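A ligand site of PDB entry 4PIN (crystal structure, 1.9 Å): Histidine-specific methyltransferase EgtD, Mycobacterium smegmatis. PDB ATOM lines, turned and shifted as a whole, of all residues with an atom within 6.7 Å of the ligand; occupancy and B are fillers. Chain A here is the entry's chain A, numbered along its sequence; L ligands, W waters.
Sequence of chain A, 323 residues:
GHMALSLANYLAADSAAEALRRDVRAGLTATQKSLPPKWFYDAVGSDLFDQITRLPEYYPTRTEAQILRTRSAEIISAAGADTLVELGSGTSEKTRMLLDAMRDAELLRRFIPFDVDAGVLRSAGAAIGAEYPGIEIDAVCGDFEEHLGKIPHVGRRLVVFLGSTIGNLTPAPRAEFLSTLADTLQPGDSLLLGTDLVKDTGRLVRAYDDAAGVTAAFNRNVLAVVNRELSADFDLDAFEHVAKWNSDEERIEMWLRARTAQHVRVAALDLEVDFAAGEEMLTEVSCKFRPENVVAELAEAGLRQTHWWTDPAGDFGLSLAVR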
ATOM      1  N   PHE A  40      21.144  17.928 -13.718  1.00  0.00           N
ATOM      2  CA  PHE A  40      21.796  19.200 -13.465  1.00  0.00           C
ATOM      3  C   PHE A  40      22.631  19.133 -12.196  1.00  0.00           C
ATOM      4  O   PHE A  40      23.619  19.835 -12.062  1.00  0.00           O
ATOM      5  CB  PHE A  40      20.773  20.343 -13.296  1.00  0.00           C
ATOM      6  CG  PHE A  40      20.194  20.856 -14.587  1.00  0.00           C
ATOM      7  CD1 PHE A  40      20.980  21.038 -15.711  1.00  0.00           C
ATOM      8  CD2 PHE A  40      18.845  21.170 -14.656  1.00  0.00           C
ATOM      9  CE1 PHE A  40      20.432  21.518 -16.885  1.00  0.00           C
ATOM     10  CE2 PHE A  40      18.298  21.649 -15.829  1.00  0.00           C
ATOM     11  CZ  PHE A  40      19.088  21.821 -16.941  1.00  0.00           C
ATOM     12  N   TYR A  41      22.212  18.282 -11.268  1.00  0.00           N
ATOM     13  CA  TYR A  41      22.626  18.428  -9.881  1.00  0.00           C
ATOM     14  C   TYR A  41      23.734  17.483  -9.444  1.00  0.00           C
ATOM     15  O   TYR A  41      23.617  16.764  -8.459  1.00  0.00           O
ATOM     16  CB  TYR A  41      21.401  18.258  -8.980  1.00  0.00           C
ATOM     17  CG  TYR A  41      20.380  19.335  -9.234  1.00  0.00           C
ATOM     18  CD1 TYR A  41      20.538  20.606  -8.715  1.00  0.00           C
ATOM     19  CD2 TYR A  41      19.250  19.089 -10.020  1.00  0.00           C
ATOM     20  CE1 TYR A  41      19.616  21.606  -8.949  1.00  0.00           C
ATOM     21  CE2 TYR A  41      18.326  20.078 -10.264  1.00  0.00           C
ATOM     22  CZ  TYR A  41      18.506  21.335  -9.732  1.00  0.00           C
ATOM     23  OH  TYR A  41      17.588  22.327  -9.968  1.00  0.00           O
ATOM     24  N   PHE A  49      23.432  26.213  -8.909  1.00  0.00           N
ATOM     25  CA  PHE A  49      22.062  26.499  -8.511  1.00  0.00           C
ATOM     26  C   PHE A  49      22.053  27.352  -7.251  1.00  0.00           C
ATOM     27  O   PHE A  49      21.245  28.270  -7.118  1.00  0.00           O
ATOM     28  CB  PHE A  49      21.242  25.234  -8.264  1.00  0.00           C
ATOM     29  CG  PHE A  49      19.862  25.526  -7.779  1.00  0.00           C
ATOM     30  CD1 PHE A  49      18.917  26.057  -8.635  1.00  0.00           C
ATOM     31  CD2 PHE A  49      19.514  25.322  -6.454  1.00  0.00           C
ATOM     32  CE1 PHE A  49      17.636  26.348  -8.193  1.00  0.00           C
ATOM     33  CE2 PHE A  49      18.238  25.615  -6.004  1.00  0.00           C
ATOM     34  CZ  PHE A  49      17.303  26.130  -6.877  1.00  0.00           C
ATOM     35  N   ILE A  52      22.429  30.701  -8.243  1.00  0.00           N
ATOM     36  CA  ILE A  52      21.220  31.206  -8.884  1.00  0.00           C
ATOM     37  C   ILE A  52      20.263  31.770  -7.830  1.00  0.00           C
ATOM     38  O   ILE A  52      19.614  32.794  -8.073  1.00  0.00           O
ATOM     39  CB  ILE A  52      20.516  30.096  -9.700  1.00  0.00           C
ATOM     40  CG1 ILE A  52      21.295  29.835 -10.985  1.00  0.00           C
ATOM     41  CG2 ILE A  52      19.080  30.504 -10.042  1.00  0.00           C
ATOM     42  CD1 ILE A  52      20.843  28.607 -11.750  1.00  0.00           C
ATOM     43  N   TYR A  58      16.446  36.281 -10.048  1.00  0.00           N
ATOM     44  CA  TYR A  58      15.786  35.084  -9.541  1.00  0.00           C
ATOM     45  C   TYR A  58      15.119  35.347  -8.190  1.00  0.00           C
ATOM     46  O   TYR A  58      15.673  35.069  -7.146  1.00  0.00           O
ATOM     47  CB  TYR A  58      16.783  33.935  -9.433  1.00  0.00           C
ATOM     48  CG  TYR A  58      16.143  32.587  -9.153  1.00  0.00           C
ATOM     49  CD1 TYR A  58      15.505  31.873 -10.164  1.00  0.00           C
ATOM     50  CD2 TYR A  58      16.188  32.023  -7.881  1.00  0.00           C
ATOM     51  CE1 TYR A  58      14.919  30.645  -9.910  1.00  0.00           C
ATOM     52  CE2 TYR A  58      15.610  30.811  -7.625  1.00  0.00           C
ATOM     53  CZ  TYR A  58      14.987  30.116  -8.640  1.00  0.00           C
ATOM     54  OH  TYR A  58      14.407  28.890  -8.379  1.00  0.00           O
ATOM     55  N   PRO A  60      12.448  33.843  -6.765  1.00  0.00           N
ATOM     56  CA  PRO A  60      11.775  32.805  -5.972  1.00  0.00           C
ATOM     57  C   PRO A  60      12.329  32.535  -4.570  1.00  0.00           C
ATOM     58  O   PRO A  60      11.544  32.521  -3.615  1.00  0.00           O
ATOM     59  CB  PRO A  60      11.928  31.566  -6.841  1.00  0.00           C
ATOM     60  CG  PRO A  60      11.921  32.084  -8.212  1.00  0.00           C
ATOM     61  CD  PRO A  60      12.707  33.368  -8.142  1.00  0.00           C
ATOM     62  N   LEU A 162       9.943  22.920  -0.612  1.00  0.00           N
ATOM     63  CA  LEU A 162      10.016  24.345  -0.893  1.00  0.00           C
ATOM     64  C   LEU A 162      10.631  24.653  -2.244  1.00  0.00           C
ATOM     65  O   LEU A 162      11.110  23.769  -2.940  1.00  0.00           O
ATOM     66  CB  LEU A 162      10.828  25.043   0.217  1.00  0.00           C
ATOM     67  CG  LEU A 162      10.328  24.794   1.642  1.00  0.00           C
ATOM     68  CD1 LEU A 162      11.288  25.399   2.654  1.00  0.00           C
ATOM     69  CD2 LEU A 162       8.927  25.350   1.841  1.00  0.00           C
ATOM     70  N   GLY A 163      10.606  25.939  -2.617  1.00  0.00           N
ATOM     71  CA  GLY A 163      11.345  26.428  -3.763  1.00  0.00           C
ATOM     72  C   GLY A 163      10.641  26.254  -5.100  1.00  0.00           C
ATOM     73  O   GLY A 163      11.188  26.620  -6.130  1.00  0.00           O
ATOM     74  N   SER A 164       9.427  25.699  -5.073  1.00  0.00           N
ATOM     75  CA  SER A 164       8.664  25.400  -6.285  1.00  0.00           C
ATOM     76  C   SER A 164       9.361  24.315  -7.106  1.00  0.00           C
ATOM     77  O   SER A 164       9.221  24.262  -8.335  1.00  0.00           O
ATOM     78  CB  SER A 164       8.463  26.650  -7.128  1.00  0.00           C
ATOM     79  OG  SER A 164       7.354  26.503  -7.986  1.00  0.00           O
ATOM     80  N   THR A 165      10.105  23.450  -6.440  1.00  0.00           N
ATOM     81  CA  THR A 165      10.687  22.287  -7.102  1.00  0.00           C
ATOM     82  C   THR A 165       9.560  21.401  -7.641  1.00  0.00           C
ATOM     83  O   THR A 165       9.760  20.660  -8.598  1.00  0.00           O
ATOM     84  CB  THR A 165      11.609  21.494  -6.139  1.00  0.00           C
ATOM     85  OG1 THR A 165      12.720  22.327  -5.772  1.00  0.00           O
ATOM     86  CG2 THR A 165      12.140  20.225  -6.795  1.00  0.00           C
ATOM     87  N   ILE A 166       8.380  21.508  -7.045  1.00  0.00           N
ATOM     88  CA  ILE A 166       7.234  20.752  -7.537  1.00  0.00           C
ATOM     89  C   ILE A 166       6.912  21.166  -8.975  1.00  0.00           C
ATOM     90  O   ILE A 166       6.394  20.380  -9.759  1.00  0.00           O
ATOM     91  CB  ILE A 166       5.985  20.954  -6.643  1.00  0.00           C
ATOM     92  CG1 ILE A 166       4.851  20.017  -7.082  1.00  0.00           C
ATOM     93  CG2 ILE A 166       5.510  22.408  -6.661  1.00  0.00           C
ATOM     94  CD1 ILE A 166       4.630  18.859  -6.151  1.00  0.00           C
ATOM     95  N   GLY A 167       7.236  22.410  -9.322  1.00  0.00           N
ATOM     96  CA  GLY A 167       7.006  22.912 -10.661  1.00  0.00           C
ATOM     97  C   GLY A 167       7.942  22.326 -11.704  1.00  0.00           C
ATOM     98  O   GLY A 167       7.737  22.496 -12.903  1.00  0.00           O
ATOM     99  N   ASN A 168       8.977  21.623 -11.249  1.00  0.00           N
ATOM    100  CA  ASN A 168       9.946  21.014 -12.166  1.00  0.00           C
ATOM    101  C   ASN A 168       9.480  19.639 -12.638  1.00  0.00           C
ATOM    102  O   ASN A 168      10.220  18.927 -13.308  1.00  0.00           O
ATOM    103  CB  ASN A 168      11.324  20.917 -11.503  1.00  0.00           C
ATOM    104  CG  ASN A 168      11.960  22.276 -11.289  1.00  0.00           C
ATOM    105  OD1 ASN A 168      12.414  22.593 -10.185  1.00  0.00           O
ATOM    106  ND2 ASN A 168      11.991  23.084 -12.334  1.00  0.00           N
ATOM    107  N   ASP A 196       5.660  28.604  -7.048  1.00  0.00           N
ATOM    108  CA  ASP A 196       5.879  29.874  -7.728  1.00  0.00           C
ATOM    109  C   ASP A 196       4.673  30.156  -8.628  1.00  0.00           C
ATOM    110  O   ASP A 196       4.130  29.237  -9.259  1.00  0.00           O
ATOM    111  CB  ASP A 196       7.173  29.843  -8.549  1.00  0.00           C
ATOM    112  CG  ASP A 196       7.605  31.222  -8.997  1.00  0.00           C
ATOM    113  OD1 ASP A 196       7.054  32.218  -8.487  1.00  0.00           O
ATOM    114  OD2 ASP A 196       8.526  31.312  -9.848  1.00  0.00           O
ATOM    115  N   ALA A 207      14.264  35.829 -14.848  1.00  0.00           N
ATOM    116  CA  ALA A 207      14.665  35.010 -13.708  1.00  0.00           C
ATOM    117  C   ALA A 207      15.372  33.732 -14.135  1.00  0.00           C
ATOM    118  O   ALA A 207      16.046  33.083 -13.326  1.00  0.00           O
ATOM    119  CB  ALA A 207      13.454  34.673 -12.852  1.00  0.00           C
ATOM    120  N   TYR A 208      15.227  33.355 -15.402  1.00  0.00           N
ATOM    121  CA  TYR A 208      15.838  32.145 -15.941  1.00  0.00           C
ATOM    122  C   TYR A 208      16.792  32.471 -17.087  1.00  0.00           C
ATOM    123  O   TYR A 208      17.160  31.599 -17.867  1.00  0.00           O
ATOM    124  CB  TYR A 208      14.750  31.165 -16.393  1.00  0.00           C
ATOM    125  CG  TYR A 208      13.955  30.656 -15.221  1.00  0.00           C
ATOM    126  CD1 TYR A 208      12.901  31.389 -14.708  1.00  0.00           C
ATOM    127  CD2 TYR A 208      14.290  29.459 -14.612  1.00  0.00           C
ATOM    128  CE1 TYR A 208      12.184  30.942 -13.620  1.00  0.00           C
ATOM    129  CE2 TYR A 208      13.571  28.999 -13.518  1.00  0.00           C
ATOM    130  CZ  TYR A 208      12.520  29.747 -13.025  1.00  0.00           C
ATOM    131  OH  TYR A 208      11.807  29.291 -11.938  1.00  0.00           O
ATOM    132  N   THR A 215      22.720  31.198 -15.024  1.00  0.00           N
ATOM    133  CA  THR A 215      21.726  30.170 -15.353  1.00  0.00           C
ATOM    134  C   THR A 215      22.151  29.437 -16.621  1.00  0.00           C
ATOM    135  O   THR A 215      22.023  28.212 -16.698  1.00  0.00           O
ATOM    136  CB  THR A 215      20.326  30.767 -15.541  1.00  0.00           C
ATOM    137  OG1 THR A 215      19.972  31.553 -14.400  1.00  0.00           O
ATOM    138  CG2 THR A 215      19.287  29.663 -15.716  1.00  0.00           C
ATOM    139  N   PHE A 218      24.602  26.911 -15.669  1.00  0.00           N
ATOM    140  CA  PHE A 218      23.855  25.850 -14.994  1.00  0.00           C
ATOM    141  C   PHE A 218      23.221  24.902 -16.008  1.00  0.00           C
ATOM    142  O   PHE A 218      23.289  23.680 -15.876  1.00  0.00           O
ATOM    143  CB  PHE A 218      22.784  26.477 -14.089  1.00  0.00           C
ATOM    144  CG  PHE A 218      21.865  25.482 -13.449  1.00  0.00           C
ATOM    145  CD1 PHE A 218      22.322  24.622 -12.464  1.00  0.00           C
ATOM    146  CD2 PHE A 218      20.522  25.442 -13.795  1.00  0.00           C
ATOM    147  CE1 PHE A 218      21.463  23.718 -11.861  1.00  0.00           C
ATOM    148  CE2 PHE A 218      19.664  24.540 -13.206  1.00  0.00           C
ATOM    149  CZ  PHE A 218      20.138  23.679 -12.235  1.00  0.00           C
ATOM    150  N   MET A 254      13.654  25.831 -20.199  1.00  0.00           N
ATOM    151  CA  MET A 254      15.059  26.062 -20.547  1.00  0.00           C
ATOM    152  C   MET A 254      15.426  25.175 -21.723  1.00  0.00           C
ATOM    153  O   MET A 254      15.156  23.969 -21.713  1.00  0.00           O
ATOM    154  CB  MET A 254      15.974  25.798 -19.355  1.00  0.00           C
ATOM    155  CG  MET A 254      15.721  26.706 -18.161  1.00  0.00           C
ATOM    156  SD  MET A 254      17.197  27.023 -17.191  1.00  0.00           S
ATOM    157  CE  MET A 254      17.798  25.353 -16.937  1.00  0.00           C
ATOM    158  N   GLU A 284      14.683  21.595 -19.196  1.00  0.00           N
ATOM    159  CA  GLU A 284      13.923  21.794 -17.962  1.00  0.00           C
ATOM    160  C   GLU A 284      12.640  22.577 -18.180  1.00  0.00           C
ATOM    161  O   GLU A 284      12.593  23.505 -18.980  1.00  0.00           O
ATOM    162  CB  GLU A 284      14.775  22.533 -16.925  1.00  0.00           C
ATOM    163  CG  GLU A 284      14.190  22.526 -15.525  1.00  0.00           C
ATOM    164  CD  GLU A 284      14.942  23.452 -14.576  1.00  0.00           C
ATOM    165  OE1 GLU A 284      15.004  24.659 -14.867  1.00  0.00           O
ATOM    166  OE2 GLU A 284      15.464  22.969 -13.553  1.00  0.00           O
ATOM    167  N   VAL A 285      11.600  22.185 -17.451  1.00  0.00           N
ATOM    168  CA  VAL A 285      10.410  23.013 -17.319  1.00  0.00           C
ATOM    169  C   VAL A 285      10.322  23.533 -15.885  1.00  0.00           C
ATOM    170  O   VAL A 285      10.761  22.863 -14.952  1.00  0.00           O
ATOM    171  CB  VAL A 285       9.113  22.255 -17.685  1.00  0.00           C
ATOM    172  CG1 VAL A 285       9.203  21.676 -19.077  1.00  0.00           C
ATOM    173  CG2 VAL A 285       8.797  21.161 -16.654  1.00  0.00           C
ATOM    174  N   SER A 286       9.780  24.730 -15.746  1.00  0.00           N
ATOM    175  CA  SER A 286       9.511  25.298 -14.429  1.00  0.00           C
ATOM    176  C   SER A 286       8.092  25.831 -14.461  1.00  0.00           C
ATOM    177  O   SER A 286       7.848  26.993 -14.803  1.00  0.00           O
ATOM    178  CB  SER A 286      10.510  26.394 -14.083  1.00  0.00           C
ATOM    179  OG  SER A 286      10.270  26.924 -12.792  1.00  0.00           O
ATOM    180  N   CYS A 287       7.141  24.951 -14.134  1.00  0.00           N
ATOM    181  CA  CYS A 287       5.724  25.278 -14.216  1.00  0.00           C
ATOM    182  C   CYS A 287       5.353  26.303 -13.157  1.00  0.00           C
ATOM    183  O   CYS A 287       5.794  26.224 -12.008  1.00  0.00           O
ATOM    184  CB  CYS A 287       4.879  24.010 -14.041  1.00  0.00           C
ATOM    185  SG  CYS A 287       5.229  22.716 -15.272  1.00  0.00           S
ATOM    186  N   LYS A 288       4.549  27.283 -13.565  1.00  0.00           N
ATOM    187  CA  LYS A 288       4.061  28.314 -12.649  1.00  0.00           C
ATOM    188  C   LYS A 288       2.567  28.120 -12.411  1.00  0.00           C
ATOM    189  O   LYS A 288       1.832  27.714 -13.309  1.00  0.00           O
ATOM    190  CB  LYS A 288       4.359  29.708 -13.204  1.00  0.00           C
ATOM    191  CG  LYS A 288       5.835  29.911 -13.577  1.00  0.00           C
ATOM    192  CD  LYS A 288       6.774  29.615 -12.396  1.00  0.00           C
ATOM    193  CE  LYS A 288       8.236  29.767 -12.782  1.00  0.00           C
ATOM    194  NZ  LYS A 288       9.140  29.329 -11.678  1.00  0.00           N
HETATM  195  C1  LIG L   1      14.802  23.793  -8.535  1.00  0.00           C
HETATM  196  N1  LIG L   1      13.757  24.564  -9.202  1.00  0.00           N
HETATM  197  C2  LIG L   1      12.911  25.127  -8.147  1.00  0.00           C
HETATM  198  C3  LIG L   1      14.350  25.688  -9.913  1.00  0.00           C
HETATM  199  C4  LIG L   1      13.263  26.531 -10.606  1.00  0.00           C
HETATM  200  O1  LIG L   1      12.567  25.919 -11.410  1.00  0.00           O
HETATM  201  O2  LIG L   1      13.149  27.723 -10.343  1.00  0.00           O
HETATM  202  C5  LIG L   1      15.358  25.230 -10.973  1.00  0.00           C
HETATM  203  C6  LIG L   1      15.981  26.364 -11.739  1.00  0.00           C
HETATM  204  N2  LIG L   1      16.258  26.292 -13.031  1.00  0.00           N
HETATM  205  C7  LIG L   1      16.807  27.411 -13.451  1.00  0.00           C
HETATM  206  N3  LIG L   1      16.885  28.237 -12.430  1.00  0.00           N
HETATM  207  C8  LIG L   1      16.378  27.601 -11.330  1.00  0.00           C
HETATM  208  O   HOH W   1       9.858  24.883 -10.942  1.00  0.00           O
HETATM  209  O   HOH W   2      17.602  30.907 -13.126  1.00  0.00           O
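The side-chain amide nitrogen of Asn 168 sits at hydrogen-bond distance from an oxygen (O1) of the ligand. The side-chain hydroxyl (OH) of Tyr 208 is in hydrogen-bond range of an oxygen (O2) of the ligand. An oxygen (O2) of the ligand lies within hydrogen-bond range of the side-chain hydroxyl of Tyr 58 (2.6 Å). N2 of the ligand is in hydrogen-bond range of OE1 of Glu 284, 2.8 Å away. O1 of the ligand is in hydrogen-bond range of OG of Ser 286, at 2.9 Å.
ND2 of Asn 168 is in hydrogen-bond range of O of Val 285. The side-chain hydroxyl of Tyr 208 sits at hydrogen-bond distance from the side-chain hydroxyl of Ser 286, at 2.9 Å. The side-chain hydroxyl (OH) of Tyr 208 lies within hydrogen-bond range of the side-chain amino group (NZ) of Lys 288. O of Glu 284 sits at hydrogen-bond distance from N of Met 254, at 2.8 Å. The side-chain amino group of Lys 288 lies within hydrogen-bond range of the side-chain hydroxyl of Ser 286 (2.9 Å). The side-chain hydroxyl (OG) of Ser 164 lies within hydrogen-bond range of the backbone NH (N) of Asp 196 (2.9 Å).
Residues that only touch the ligand: Tyr 41, Phe 49, Ile 52, Gly 163, Ser 164, Thr 165, Phe 218 and Met 254. Hydrophobic or aromatic side chains that line the ligand: Phe 49, Ile 52, Tyr 58, Tyr 208, Phe 218 and Met 254. 13 residues have an atom within 4 Å of the ligand: Tyr 41, Phe 49, Ile 52, Tyr 58, Gly 163, Ser 164, Thr 165, Asn 168, Tyr 208, Phe 218, Met 254, Glu 284 and Ser 286. The nearest printed residue that does not touch the ligand is Thr 215 (4.04 Å).
Water W2 lies within hydrogen-bond range of the backbone carbonyl oxygen of Ala 207, the side-chain hydroxyl of Thr 215 and a nitrogen (N3) of the ligand. Water W1 lies within hydrogen-bond range of the backbone carbonyl oxygen of Ser 164 (2.8 Å), the side-chain hydroxyl of Ser 286 (2.8 Å), an oxygen (O1) of the ligand (2.9 Å) and the side-chain amide nitrogen of Asn 168 (3.1 Å).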
